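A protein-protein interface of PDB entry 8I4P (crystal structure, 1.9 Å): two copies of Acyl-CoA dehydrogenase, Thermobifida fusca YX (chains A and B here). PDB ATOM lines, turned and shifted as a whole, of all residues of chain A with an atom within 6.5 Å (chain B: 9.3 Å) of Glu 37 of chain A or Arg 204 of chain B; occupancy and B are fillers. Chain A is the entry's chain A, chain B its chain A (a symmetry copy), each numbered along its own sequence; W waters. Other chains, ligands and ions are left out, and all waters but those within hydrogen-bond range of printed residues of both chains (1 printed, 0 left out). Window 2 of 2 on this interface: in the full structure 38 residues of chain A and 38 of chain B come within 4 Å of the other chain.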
ATOM      1  N   ALA A  32      14.768  -7.852  -8.217  1.00  0.00           N
ATOM      2  CA  ALA A  32      13.487  -8.314  -7.648  1.00  0.00           C
ATOM      3  C   ALA A  32      12.481  -8.482  -8.781  1.00  0.00           C
ATOM      4  O   ALA A  32      11.762  -9.487  -8.801  1.00  0.00           O
ATOM      5  CB  ALA A  32      12.992  -7.341  -6.592  1.00  0.00           C
ATOM      6  N   ALA A  33      12.379  -7.510  -9.691  1.00  0.00           N
ATOM      7  CA  ALA A  33      11.359  -7.573 -10.773  1.00  0.00           C
ATOM      8  C   ALA A  33      11.623  -8.765 -11.695  1.00  0.00           C
ATOM      9  O   ALA A  33      10.662  -9.498 -12.077  1.00  0.00           O
ATOM     10  CB  ALA A  33      11.324  -6.280 -11.565  1.00  0.00           C
ATOM     11  N   ASP A  34      12.891  -8.970 -12.056  1.00  0.00           N
ATOM     12  CA  ASP A  34      13.273 -10.077 -12.964  1.00  0.00           C
ATOM     13  C   ASP A  34      13.067 -11.431 -12.276  1.00  0.00           C
ATOM     14  O   ASP A  34      12.563 -12.415 -12.919  1.00  0.00           O
ATOM     15  CB  ASP A  34      14.709  -9.874 -13.423  1.00  0.00           C
ATOM     16  CG  ASP A  34      15.070 -10.868 -14.491  1.00  0.00           C
ATOM     17  OD1 ASP A  34      14.456 -10.783 -15.590  1.00  0.00           O
ATOM     18  OD2 ASP A  34      15.801 -11.823 -14.140  1.00  0.00           O
ATOM     19  N   VAL A  35      13.375 -11.508 -10.992  1.00  0.00           N
ATOM     20  CA  VAL A  35      13.123 -12.737 -10.182  1.00  0.00           C
ATOM     21  C   VAL A  35      11.638 -13.172 -10.225  1.00  0.00           C
ATOM     22  O   VAL A  35      11.332 -14.383 -10.457  1.00  0.00           O
ATOM     23  CB  VAL A  35      13.626 -12.504  -8.750  1.00  0.00           C
ATOM     24  CG1 VAL A  35      13.022 -13.477  -7.749  1.00  0.00           C
ATOM     25  CG2 VAL A  35      15.147 -12.613  -8.742  1.00  0.00           C
ATOM     26  N   ASP A  36      10.737 -12.217 -10.020  1.00  0.00           N
ATOM     27  CA  ASP A  36       9.262 -12.414 -10.116  1.00  0.00           C
ATOM     28  C   ASP A  36       8.898 -12.782 -11.566  1.00  0.00           C
ATOM     29  O   ASP A  36       8.154 -13.770 -11.784  1.00  0.00           O
ATOM     30  CB  ASP A  36       8.562 -11.116  -9.643  1.00  0.00           C
ATOM     31  CG  ASP A  36       7.067 -11.138  -9.923  1.00  0.00           C
ATOM     32  OD1 ASP A  36       6.370 -11.889  -9.224  1.00  0.00           O
ATOM     33  OD2 ASP A  36       6.652 -10.541 -10.940  1.00  0.00           O
ATOM     34  N   GLU A  37       9.331 -11.948 -12.522  1.00  0.00           N
ATOM     35  CA  GLU A  37       8.894 -12.037 -13.942  1.00  0.00           C
ATOM     36  C   GLU A  37       9.321 -13.383 -14.547  1.00  0.00           C
ATOM     37  O   GLU A  37       8.514 -13.981 -15.242  1.00  0.00           O
ATOM     38  CB  GLU A  37       9.473 -10.891 -14.767  1.00  0.00           C
ATOM     39  CG  GLU A  37       8.824 -10.795 -16.124  1.00  0.00           C
ATOM     40  CD  GLU A  37       7.404 -10.255 -16.075  1.00  0.00           C
ATOM     41  OE1 GLU A  37       6.869 -10.013 -14.947  1.00  0.00           O
ATOM     42  OE2 GLU A  37       6.840 -10.003 -17.170  1.00  0.00           O
ATOM     43  N   GLN A  38      10.506 -13.902 -14.210  1.00  0.00           N
ATOM     44  CA  GLN A  38      11.001 -15.203 -14.755  1.00  0.00           C
ATOM     45  C   GLN A  38      10.735 -16.338 -13.777  1.00  0.00           C
ATOM     46  O   GLN A  38      11.165 -17.448 -14.065  1.00  0.00           O
ATOM     47  CB  GLN A  38      12.500 -15.118 -15.034  1.00  0.00           C
ATOM     48  CG  GLN A  38      12.912 -14.004 -16.008  1.00  0.00           C
ATOM     49  CD  GLN A  38      12.094 -14.050 -17.274  1.00  0.00           C
ATOM     50  OE1 GLN A  38      11.814 -15.117 -17.824  1.00  0.00           O
ATOM     51  NE2 GLN A  38      11.639 -12.892 -17.719  1.00  0.00           N
ATOM     52  N   SER A  39      10.116 -16.075 -12.630  1.00  0.00           N
ATOM     53  CA  SER A  39       9.841 -17.097 -11.599  1.00  0.00           C
ATOM     54  C   SER A  39      11.126 -17.874 -11.304  1.00  0.00           C
ATOM     55  O   SER A  39      11.064 -19.093 -11.345  1.00  0.00           O
ATOM     56  CB  SER A  39       8.734 -18.054 -12.012  1.00  0.00           C
ATOM     57  OG  SER A  39       7.499 -17.343 -12.192  1.00  0.00           O
ATOM     58  N   ARG A  40      12.238 -17.195 -11.051  1.00  0.00           N
ATOM     59  CA  ARG A  40      13.552 -17.868 -10.934  1.00  0.00           C
ATOM     60  C   ARG A  40      14.093 -17.603  -9.528  1.00  0.00           C
ATOM     61  O   ARG A  40      13.870 -16.519  -8.957  1.00  0.00           O
ATOM     62  CB  ARG A  40      14.486 -17.357 -12.044  1.00  0.00           C
ATOM     63  CG  ARG A  40      15.015 -15.958 -11.770  1.00  0.00           C
ATOM     64  CD  ARG A  40      15.989 -15.443 -12.763  1.00  0.00           C
ATOM     65  NE  ARG A  40      16.316 -14.017 -12.660  1.00  0.00           N
ATOM     66  CZ  ARG A  40      17.207 -13.487 -11.848  1.00  0.00           C
ATOM     67  NH1 ARG A  40      17.792 -14.193 -10.891  1.00  0.00           N
ATOM     68  NH2 ARG A  40      17.464 -12.205 -11.953  1.00  0.00           N
ATOM     69  N   LYS A 209       7.146 -15.490  -6.621  1.00  0.00           N
ATOM     70  CA  LYS A 209       7.283 -16.345  -7.813  1.00  0.00           C
ATOM     71  C   LYS A 209       8.720 -16.863  -7.959  1.00  0.00           C
ATOM     72  O   LYS A 209       8.847 -17.955  -8.450  1.00  0.00           O
ATOM     73  CB  LYS A 209       6.819 -15.629  -9.074  1.00  0.00           C
ATOM     74  CG  LYS A 209       5.325 -15.412  -9.074  1.00  0.00           C
ATOM     75  CD  LYS A 209       4.850 -14.613 -10.246  1.00  0.00           C
ATOM     76  CE  LYS A 209       4.874 -15.430 -11.490  1.00  0.00           C
ATOM     77  NZ  LYS A 209       4.015 -14.790 -12.506  1.00  0.00           N
ATOM     78  N   TYR A 348      -1.079  -0.643 -11.449  1.00  0.00           N
ATOM     79  CA  TYR A 348      -1.628  -1.915 -11.983  1.00  0.00           C
ATOM     80  C   TYR A 348      -0.627  -2.518 -12.983  1.00  0.00           C
ATOM     81  O   TYR A 348      -0.949  -3.600 -13.549  1.00  0.00           O
ATOM     82  CB  TYR A 348      -2.994  -1.620 -12.622  1.00  0.00           C
ATOM     83  CG  TYR A 348      -3.858  -2.826 -12.742  1.00  0.00           C
ATOM     84  CD1 TYR A 348      -4.472  -3.361 -11.618  1.00  0.00           C
ATOM     85  CD2 TYR A 348      -4.084  -3.443 -13.957  1.00  0.00           C
ATOM     86  CE1 TYR A 348      -5.285  -4.477 -11.694  1.00  0.00           C
ATOM     87  CE2 TYR A 348      -4.911  -4.560 -14.048  1.00  0.00           C
ATOM     88  CZ  TYR A 348      -5.513  -5.084 -12.922  1.00  0.00           C
ATOM     89  OH  TYR A 348      -6.305  -6.204 -12.986  1.00  0.00           O
ATOM     90  N   THR A 349       0.520  -1.856 -13.245  1.00  0.00           N
ATOM     91  CA  THR A 349       1.484  -2.350 -14.246  1.00  0.00           C
ATOM     92  C   THR A 349       2.733  -2.897 -13.578  1.00  0.00           C
ATOM     93  O   THR A 349       3.091  -2.424 -12.494  1.00  0.00           O
ATOM     94  CB  THR A 349       1.841  -1.294 -15.279  1.00  0.00           C
ATOM     95  OG1 THR A 349       2.667  -0.345 -14.629  1.00  0.00           O
ATOM     96  CG2 THR A 349       0.604  -0.662 -15.876  1.00  0.00           C
ATOM     97  N   ARG A 350       3.396  -3.816 -14.262  1.00  0.00           N
ATOM     98  CA  ARG A 350       4.547  -4.568 -13.683  1.00  0.00           C
ATOM     99  C   ARG A 350       5.783  -3.717 -13.816  1.00  0.00           C
ATOM    100  O   ARG A 350       6.803  -4.138 -13.300  1.00  0.00           O
ATOM    101  CB  ARG A 350       4.760  -5.939 -14.305  1.00  0.00           C
ATOM    102  CG  ARG A 350       3.504  -6.785 -14.182  1.00  0.00           C
ATOM    103  CD  ARG A 350       3.746  -8.278 -14.004  1.00  0.00           C
ATOM    104  NE  ARG A 350       4.283  -8.901 -15.197  1.00  0.00           N
ATOM    105  CZ  ARG A 350       3.574  -9.267 -16.275  1.00  0.00           C
ATOM    106  NH1 ARG A 350       2.271  -9.028 -16.357  1.00  0.00           N
ATOM    107  NH2 ARG A 350       4.179  -9.853 -17.299  1.00  0.00           N
ATOM    108  N   ASP A 351       5.645  -2.552 -14.418  1.00  0.00           N
ATOM    109  CA  ASP A 351       6.723  -1.545 -14.509  1.00  0.00           C
ATOM    110  C   ASP A 351       6.954  -0.871 -13.149  1.00  0.00           C
ATOM    111  O   ASP A 351       7.981  -0.179 -13.000  1.00  0.00           O
ATOM    112  CB  ASP A 351       6.351  -0.415 -15.479  1.00  0.00           C
ATOM    113  CG  ASP A 351       6.291  -0.716 -16.983  1.00  0.00           C
ATOM    114  OD1 ASP A 351       6.558  -1.853 -17.420  1.00  0.00           O
ATOM    115  OD2 ASP A 351       5.990   0.226 -17.708  1.00  0.00           O
ATOM    116  N   GLU A 355       2.385  -3.750  -7.568  1.00  0.00           N
ATOM    117  CA  GLU A 355       1.509  -4.906  -7.869  1.00  0.00           C
ATOM    118  C   GLU A 355       2.203  -6.203  -7.416  1.00  0.00           C
ATOM    119  O   GLU A 355       1.500  -7.108  -6.925  1.00  0.00           O
ATOM    120  CB  GLU A 355       1.000  -4.903  -9.320  1.00  0.00           C
ATOM    121  CG  GLU A 355       1.983  -5.211 -10.430  1.00  0.00           C
ATOM    122  CD  GLU A 355       2.409  -6.637 -10.646  1.00  0.00           C
ATOM    123  OE1 GLU A 355       3.618  -6.849 -10.898  1.00  0.00           O
ATOM    124  OE2 GLU A 355       1.524  -7.527 -10.561  1.00  0.00           O
ATOM    125  N   ARG A 359       0.777  -8.974  -4.635  1.00  0.00           N
ATOM    126  CA  ARG A 359       0.689 -10.439  -4.928  1.00  0.00           C
ATOM    127  C   ARG A 359       1.494 -11.204  -3.856  1.00  0.00           C
ATOM    128  O   ARG A 359       1.022 -12.252  -3.354  1.00  0.00           O
ATOM    129  CB  ARG A 359       1.152 -10.724  -6.356  1.00  0.00           C
ATOM    130  CG  ARG A 359       0.283 -10.085  -7.439  1.00  0.00           C
ATOM    131  CD  ARG A 359       0.758 -10.582  -8.813  1.00  0.00           C
ATOM    132  NE  ARG A 359       1.904  -9.840  -9.343  1.00  0.00           N
ATOM    133  CZ  ARG A 359       3.145 -10.335  -9.504  1.00  0.00           C
ATOM    134  NH1 ARG A 359       3.458 -11.547  -9.069  1.00  0.00           N
ATOM    135  NH2 ARG A 359       4.088  -9.593 -10.054  1.00  0.00           N
ATOM    136  N   GLU B  37      -2.998 -16.313 -18.828  1.00  0.00           N
ATOM    137  CA  GLU B  37      -1.624 -16.884 -18.784  1.00  0.00           C
ATOM    138  C   GLU B  37      -0.811 -16.409 -19.998  1.00  0.00           C
ATOM    139  O   GLU B  37       0.344 -16.056 -19.813  1.00  0.00           O
ATOM    140  CB  GLU B  37      -1.664 -18.408 -18.750  1.00  0.00           C
ATOM    141  CG  GLU B  37      -0.316 -18.996 -18.418  1.00  0.00           C
ATOM    142  CD  GLU B  37       0.079 -18.815 -16.962  1.00  0.00           C
ATOM    143  OE1 GLU B  37      -0.681 -18.146 -16.191  1.00  0.00           O
ATOM    144  OE2 GLU B  37       1.117 -19.401 -16.563  1.00  0.00           O
ATOM    145  N   SER B  39      -1.674 -13.670 -21.815  1.00  0.00           N
ATOM    146  CA  SER B  39      -1.984 -12.236 -21.987  1.00  0.00           C
ATOM    147  C   SER B  39      -2.503 -11.998 -23.406  1.00  0.00           C
ATOM    148  O   SER B  39      -1.972 -11.110 -24.054  1.00  0.00           O
ATOM    149  CB  SER B  39      -0.783 -11.346 -21.712  1.00  0.00           C
ATOM    150  OG  SER B  39      -0.355 -11.489 -20.349  1.00  0.00           O
ATOM    151  N   TRP B 159      -3.555   4.019 -21.675  1.00  0.00           N
ATOM    152  CA  TRP B 159      -4.348   3.008 -20.939  1.00  0.00           C
ATOM    153  C   TRP B 159      -5.526   2.523 -21.778  1.00  0.00           C
ATOM    154  O   TRP B 159      -6.562   2.192 -21.154  1.00  0.00           O
ATOM    155  CB  TRP B 159      -4.900   3.592 -19.605  1.00  0.00           C
ATOM    156  CG  TRP B 159      -3.883   4.192 -18.679  1.00  0.00           C
ATOM    157  CD1 TRP B 159      -3.766   5.492 -18.275  1.00  0.00           C
ATOM    158  CD2 TRP B 159      -2.751   3.499 -18.143  1.00  0.00           C
ATOM    159  NE1 TRP B 159      -2.666   5.636 -17.472  1.00  0.00           N
ATOM    160  CE2 TRP B 159      -2.014   4.436 -17.391  1.00  0.00           C
ATOM    161  CE3 TRP B 159      -2.318   2.189 -18.218  1.00  0.00           C
ATOM    162  CZ2 TRP B 159      -0.876   4.084 -16.688  1.00  0.00           C
ATOM    163  CZ3 TRP B 159      -1.186   1.835 -17.534  1.00  0.00           C
ATOM    164  CH2 TRP B 159      -0.452   2.783 -16.811  1.00  0.00           C
ATOM    165  N   GLU B 201       3.531  -0.245 -27.000  1.00  0.00           N
ATOM    166  CA  GLU B 201       3.680  -1.674 -26.602  1.00  0.00           C
ATOM    167  C   GLU B 201       2.590  -2.032 -25.601  1.00  0.00           C
ATOM    168  O   GLU B 201       2.163  -1.200 -24.832  1.00  0.00           O
ATOM    169  CB  GLU B 201       5.080  -1.824 -26.020  1.00  0.00           C
ATOM    170  CG  GLU B 201       6.143  -1.720 -27.108  1.00  0.00           C
ATOM    171  CD  GLU B 201       7.522  -2.152 -26.653  1.00  0.00           C
ATOM    172  OE1 GLU B 201       7.661  -2.366 -25.446  1.00  0.00           O
ATOM    173  OE2 GLU B 201       8.449  -2.263 -27.490  1.00  0.00           O
ATOM    174  N   PRO B 202       2.019  -3.242 -25.627  1.00  0.00           N
ATOM    175  CA  PRO B 202       0.984  -3.596 -24.659  1.00  0.00           C
ATOM    176  C   PRO B 202       1.503  -3.473 -23.205  1.00  0.00           C
ATOM    177  O   PRO B 202       2.641  -3.855 -22.954  1.00  0.00           O
ATOM    178  CB  PRO B 202       0.643  -5.058 -24.980  1.00  0.00           C
ATOM    179  CG  PRO B 202       1.206  -5.288 -26.377  1.00  0.00           C
ATOM    180  CD  PRO B 202       2.375  -4.341 -26.531  1.00  0.00           C
ATOM    181  N   GLU B 203       0.685  -2.929 -22.298  1.00  0.00           N
ATOM    182  CA  GLU B 203       1.065  -2.792 -20.871  1.00  0.00           C
ATOM    183  C   GLU B 203       1.151  -4.208 -20.298  1.00  0.00           C
ATOM    184  O   GLU B 203       0.371  -5.078 -20.736  1.00  0.00           O
ATOM    185  CB  GLU B 203       0.059  -1.993 -20.048  1.00  0.00           C
ATOM    186  CG  GLU B 203      -0.218  -0.603 -20.562  1.00  0.00           C
ATOM    187  CD  GLU B 203       0.957   0.338 -20.494  1.00  0.00           C
ATOM    188  OE1 GLU B 203       1.841   0.100 -19.630  1.00  0.00           O
ATOM    189  OE2 GLU B 203       0.946   1.312 -21.306  1.00  0.00           O
ATOM    190  N   ARG B 204       2.074  -4.420 -19.378  1.00  0.00           N
ATOM    191  CA  ARG B 204       2.202  -5.685 -18.595  1.00  0.00           C
ATOM    192  C   ARG B 204       1.483  -5.443 -17.263  1.00  0.00           C
ATOM    193  O   ARG B 204       1.899  -4.571 -16.531  1.00  0.00           O
ATOM    194  CB  ARG B 204       3.693  -6.034 -18.450  1.00  0.00           C
ATOM    195  CG  ARG B 204       4.491  -6.013 -19.748  1.00  0.00           C
ATOM    196  CD  ARG B 204       5.944  -5.564 -19.564  1.00  0.00           C
ATOM    197  NE  ARG B 204       6.561  -6.460 -18.618  1.00  0.00           N
ATOM    198  CZ  ARG B 204       7.265  -6.124 -17.524  1.00  0.00           C
ATOM    199  NH1 ARG B 204       7.563  -4.861 -17.218  1.00  0.00           N
ATOM    200  NH2 ARG B 204       7.650  -7.102 -16.722  1.00  0.00           N
ATOM    201  N   LYS B 205       0.321  -6.044 -17.084  1.00  0.00           N
ATOM    202  CA  LYS B 205      -0.664  -5.714 -16.026  1.00  0.00           C
ATOM    203  C   LYS B 205      -0.654  -6.757 -14.910  1.00  0.00           C
ATOM    204  O   LYS B 205      -0.299  -7.927 -15.167  1.00  0.00           O
ATOM    205  CB  LYS B 205      -2.044  -5.556 -16.644  1.00  0.00           C
ATOM    206  CG  LYS B 205      -2.037  -4.507 -17.754  1.00  0.00           C
ATOM    207  CD  LYS B 205      -3.360  -3.971 -18.047  1.00  0.00           C
ATOM    208  CE  LYS B 205      -4.407  -5.005 -18.391  1.00  0.00           C
ATOM    209  NZ  LYS B 205      -4.101  -5.643 -19.669  1.00  0.00           N
ATOM    210  N   LEU B 206      -1.211  -6.380 -13.762  1.00  0.00           N
ATOM    211  CA  LEU B 206      -1.511  -7.328 -12.636  1.00  0.00           C
ATOM    212  C   LEU B 206      -2.587  -8.319 -13.071  1.00  0.00           C
ATOM    213  O   LEU B 206      -2.437  -9.524 -12.845  1.00  0.00           O
ATOM    214  CB  LEU B 206      -1.993  -6.473 -11.472  1.00  0.00           C
ATOM    215  CG  LEU B 206      -2.617  -7.190 -10.268  1.00  0.00           C
ATOM    216  CD1 LEU B 206      -1.642  -8.207  -9.672  1.00  0.00           C
ATOM    217  CD2 LEU B 206      -2.986  -6.148  -9.192  1.00  0.00           C
ATOM    218  N   GLY B 207      -3.668  -7.818 -13.663  1.00  0.00           N
ATOM    219  CA  GLY B 207      -4.827  -8.638 -14.100  1.00  0.00           C
ATOM    220  C   GLY B 207      -5.443  -8.069 -15.376  1.00  0.00           C
ATOM    221  O   GLY B 207      -4.784  -7.210 -16.003  1.00  0.00           O
ATOM    222  N   ILE B 208      -6.650  -8.517 -15.706  1.00  0.00           N
ATOM    223  CA  ILE B 208      -7.286  -8.443 -17.036  1.00  0.00           C
ATOM    224  C   ILE B 208      -6.190  -8.497 -18.092  1.00  0.00           C
ATOM    225  O   ILE B 208      -6.121  -7.626 -18.995  1.00  0.00           O
ATOM    226  CB  ILE B 208      -8.227  -7.234 -17.155  1.00  0.00           C
ATOM    227  CG1 ILE B 208      -7.585  -5.915 -16.734  1.00  0.00           C
ATOM    228  CG2 ILE B 208      -9.467  -7.509 -16.363  1.00  0.00           C
ATOM    229  CD1 ILE B 208      -8.322  -4.705 -17.320  1.00  0.00           C
ATOM    230  N   LYS B 209      -5.391  -9.549 -18.010  1.00  0.00           N
ATOM    231  CA  LYS B 209      -4.164  -9.654 -18.820  1.00  0.00           C
ATOM    232  C   LYS B 209      -4.496  -9.913 -20.295  1.00  0.00           C
ATOM    233  O   LYS B 209      -3.738  -9.445 -21.104  1.00  0.00           O
ATOM    234  CB  LYS B 209      -3.216 -10.711 -18.269  1.00  0.00           C
ATOM    235  CG  LYS B 209      -2.624 -10.293 -16.944  1.00  0.00           C
ATOM    236  CD  LYS B 209      -1.774 -11.355 -16.322  1.00  0.00           C
ATOM    237  CE  LYS B 209      -0.470 -11.473 -17.028  1.00  0.00           C
ATOM    238  NZ  LYS B 209       0.488 -12.183 -16.158  1.00  0.00           N
ATOM    239  N   SER B 211      -6.980  -8.586 -21.913  1.00  0.00           N
ATOM    240  CA  SER B 211      -7.489  -7.290 -22.432  1.00  0.00           C
ATOM    241  C   SER B 211      -6.303  -6.454 -22.860  1.00  0.00           C
ATOM    242  O   SER B 211      -5.513  -6.001 -22.019  1.00  0.00           O
ATOM    243  CB  SER B 211      -8.375  -6.540 -21.453  1.00  0.00           C
ATOM    244  OG  SER B 211      -8.980  -5.428 -22.112  1.00  0.00           O
ATOM    245  N   PRO B 212      -6.133  -6.170 -24.170  1.00  0.00           N
ATOM    246  CA  PRO B 212      -5.029  -5.318 -24.600  1.00  0.00           C
ATOM    247  C   PRO B 212      -5.209  -3.915 -24.015  1.00  0.00           C
ATOM    248  O   PRO B 212      -6.342  -3.383 -24.001  1.00  0.00           O
ATOM    249  CB  PRO B 212      -5.130  -5.327 -26.142  1.00  0.00           C
ATOM    250  CG  PRO B 212      -5.987  -6.518 -26.441  1.00  0.00           C
ATOM    251  CD  PRO B 212      -6.982  -6.574 -25.298  1.00  0.00           C
ATOM    252  N   THR B 213      -4.115  -3.348 -23.508  1.00  0.00           N
ATOM    253  CA  THR B 213      -4.106  -2.016 -22.898  1.00  0.00           C
ATOM    254  C   THR B 213      -2.916  -1.273 -23.481  1.00  0.00           C
ATOM    255  O   THR B 213      -1.785  -1.711 -23.268  1.00  0.00           O
ATOM    256  CB  THR B 213      -4.082  -2.111 -21.353  1.00  0.00           C
ATOM    257  OG1 THR B 213      -5.114  -2.997 -20.899  1.00  0.00           O
ATOM    258  CG2 THR B 213      -4.303  -0.753 -20.753  1.00  0.00           C
ATOM    259  N   ARG B 214      -3.138  -0.211 -24.237  1.00  0.00           N
ATOM    260  CA  ARG B 214      -2.035   0.314 -25.098  1.00  0.00           C
ATOM    261  C   ARG B 214      -2.203   1.808 -25.242  1.00  0.00           C
ATOM    262  O   ARG B 214      -3.357   2.277 -25.221  1.00  0.00           O
ATOM    263  CB  ARG B 214      -2.023  -0.333 -26.492  1.00  0.00           C
ATOM    264  CG  ARG B 214      -2.181  -1.849 -26.459  1.00  0.00           C
ATOM    265  CD  ARG B 214      -2.014  -2.565 -27.775  1.00  0.00           C
ATOM    266  NE  ARG B 214      -0.701  -2.343 -28.374  1.00  0.00           N
ATOM    267  CZ  ARG B 214      -0.357  -2.816 -29.576  1.00  0.00           C
ATOM    268  NH1 ARG B 214      -1.212  -3.583 -30.241  1.00  0.00           N
ATOM    269  NH2 ARG B 214       0.806  -2.482 -30.109  1.00  0.00           N
ATOM    270  N   ARG B 350      -2.051 -20.934  -9.766  1.00  0.00           N
ATOM    271  CA  ARG B 350      -2.747 -20.502 -11.012  1.00  0.00           C
ATOM    272  C   ARG B 350      -3.527 -21.674 -11.549  1.00  0.00           C
ATOM    273  O   ARG B 350      -4.241 -21.468 -12.514  1.00  0.00           O
ATOM    274  CB  ARG B 350      -1.815 -19.938 -12.072  1.00  0.00           C
ATOM    275  CG  ARG B 350      -1.020 -18.767 -11.518  1.00  0.00           C
ATOM    276  CD  ARG B 350      -0.697 -17.672 -12.526  1.00  0.00           C
ATOM    277  NE  ARG B 350       0.261 -18.100 -13.527  1.00  0.00           N
ATOM    278  CZ  ARG B 350       1.589 -18.170 -13.357  1.00  0.00           C
ATOM    279  NH1 ARG B 350       2.153 -17.889 -12.190  1.00  0.00           N
ATOM    280  NH2 ARG B 350       2.366 -18.557 -14.361  1.00  0.00           N
HETATM  281  O   HOH W   1       8.321  -7.254 -14.159  1.00  0.00           O
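Of the 17 printed residues of chain B, 8 touch a printed residue of chain A.
Printed residues of chain A that touch a printed residue of chain B: Glu 37, Lys 209, Tyr 348, Thr 349, Arg 350, Asp 351, Glu 355 and Arg 359.
Among the printed residues, 14 pairs touch across the chains.
Among the printed residues, Asp or Glu carboxylates within 4 Å of a Lys or Arg side-chain nitrogen of the other chain: Glu 37 of chain A with Arg 204 of chain B (3.0 Å) and Asp 351 of chain A with Arg 204 of chain B (3.2 Å).
OE2 of Glu 37 of chain A lies within salt-bridge range of NH2 of Arg 204 of chain B (3.0 Å).
The backbone carbonyl oxygen (O) of Tyr 348 of chain A is in hydrogen-bond range of the backbone NH (N) of Leu 206 of chain B (2.8 Å).
N of Gly 207 of chain B lies close to OH of Tyr 348 of chain A (3.2 Å).
The backbone carbonyl oxygen (O) of Arg 204 of chain B lies within hydrogen-bond range of the backbone NH (N) of Arg 350 of chain A (2.8 Å).
The guanidinium group (NH1) of Arg 350 of chain A is in hydrogen-bond range of the backbone carbonyl oxygen (O) of Lys 205 of chain B, 3.0 Å away.
OD1 of Asp 351 of chain A lies within salt-bridge range of NH1 of Arg 204 of chain B, at 3.2 Å.
Water W1 lies within hydrogen-bond range of NH2 of Arg 204 of chain B and OE1 of Glu 37 of chain A.
Lys 209 of chain A touches Arg 350 of chain B, and with the chains exchanged Arg 350 of chain A touches Lys 209 of chain B.
Of the 14 pairs that touch across the chains among the printed residues, 2 have their exchanged pair printed and touching as well.
The side-chain carboxylate of Asp 36 of chain A lies within salt-bridge range of the guanidinium group of Arg 359 of chain A.
The side-chain carboxylate (OE2) of Glu 37 of chain A lies within salt-bridge range of the guanidinium group (NH2) of Arg 350 of chain A (2.7 Å).
The guanidinium group of Arg 359 of chain A is in salt-bridge range of the side-chain carboxylate of Glu 355 of chain A (2.6 Å).
NZ of Lys 205 of chain B lies within hydrogen-bond range of O of Ile 208 of chain B (2.9 Å).
The side-chain amino group of Lys 205 of chain B sits at hydrogen-bond distance from the backbone carbonyl oxygen of Ser 211 of chain B (2.8 Å).
OG1 of Thr 213 of chain B sits at hydrogen-bond distance from NZ of Lys 205 of chain B, at 3.1 Å.
Asp 34 of chain A touches none of the printed residues of chain B.
Of chain B, only Arg 204 comes within 4 Å of Glu 37 of chain A.
Of chain B, only Trp 159 and Arg 204 come within 4 Å of Thr 349 of chain A.
Arg 204 of chain B touches just these residues of chain A: Glu 37 (3.0 Å), Thr 349 (3.2 Å), Arg 350 (2.8 Å) and Asp 351 (3.2 Å).
Of the printed residues of chain A, Ile 208 of chain B touches Tyr 348 (3.6 Å).
Of the printed residues of chain A, Arg 350 of chain B touches Lys 209.
The nearest residue of chain B that does not touch Glu 37 of chain A is Lys 209 of chain B (6.8 Å).
The nearest residue of chain A that does not touch Arg 204 of chain B is Tyr 348 of chain A (4.2 Å).
The nearest printed residue of chain A that does not touch Lys 205 of chain B is Thr 349 of chain A (4.4 Å).
Lys 209 of chain A touches Arg 350 of chain B.
O of Tyr 348 of chain A touches CA of Lys 205 of chain B (3.3 Å).
Tyr 348 of chain A touches Ile 208 of chain B.
Trp 159 of chain B touches Thr 349 of chain A (CZ3 to CG2, 3.5 Å).
Thr 349 of chain A touches Arg 204 of chain B.
NZ of Lys 209 of chain B touches NH1 of Arg 350 of chain A, 3.6 Å away.
Glu 355 of chain A touches Leu 206 of chain B.
Arg 359 of chain A touches Leu 206 of chain B.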
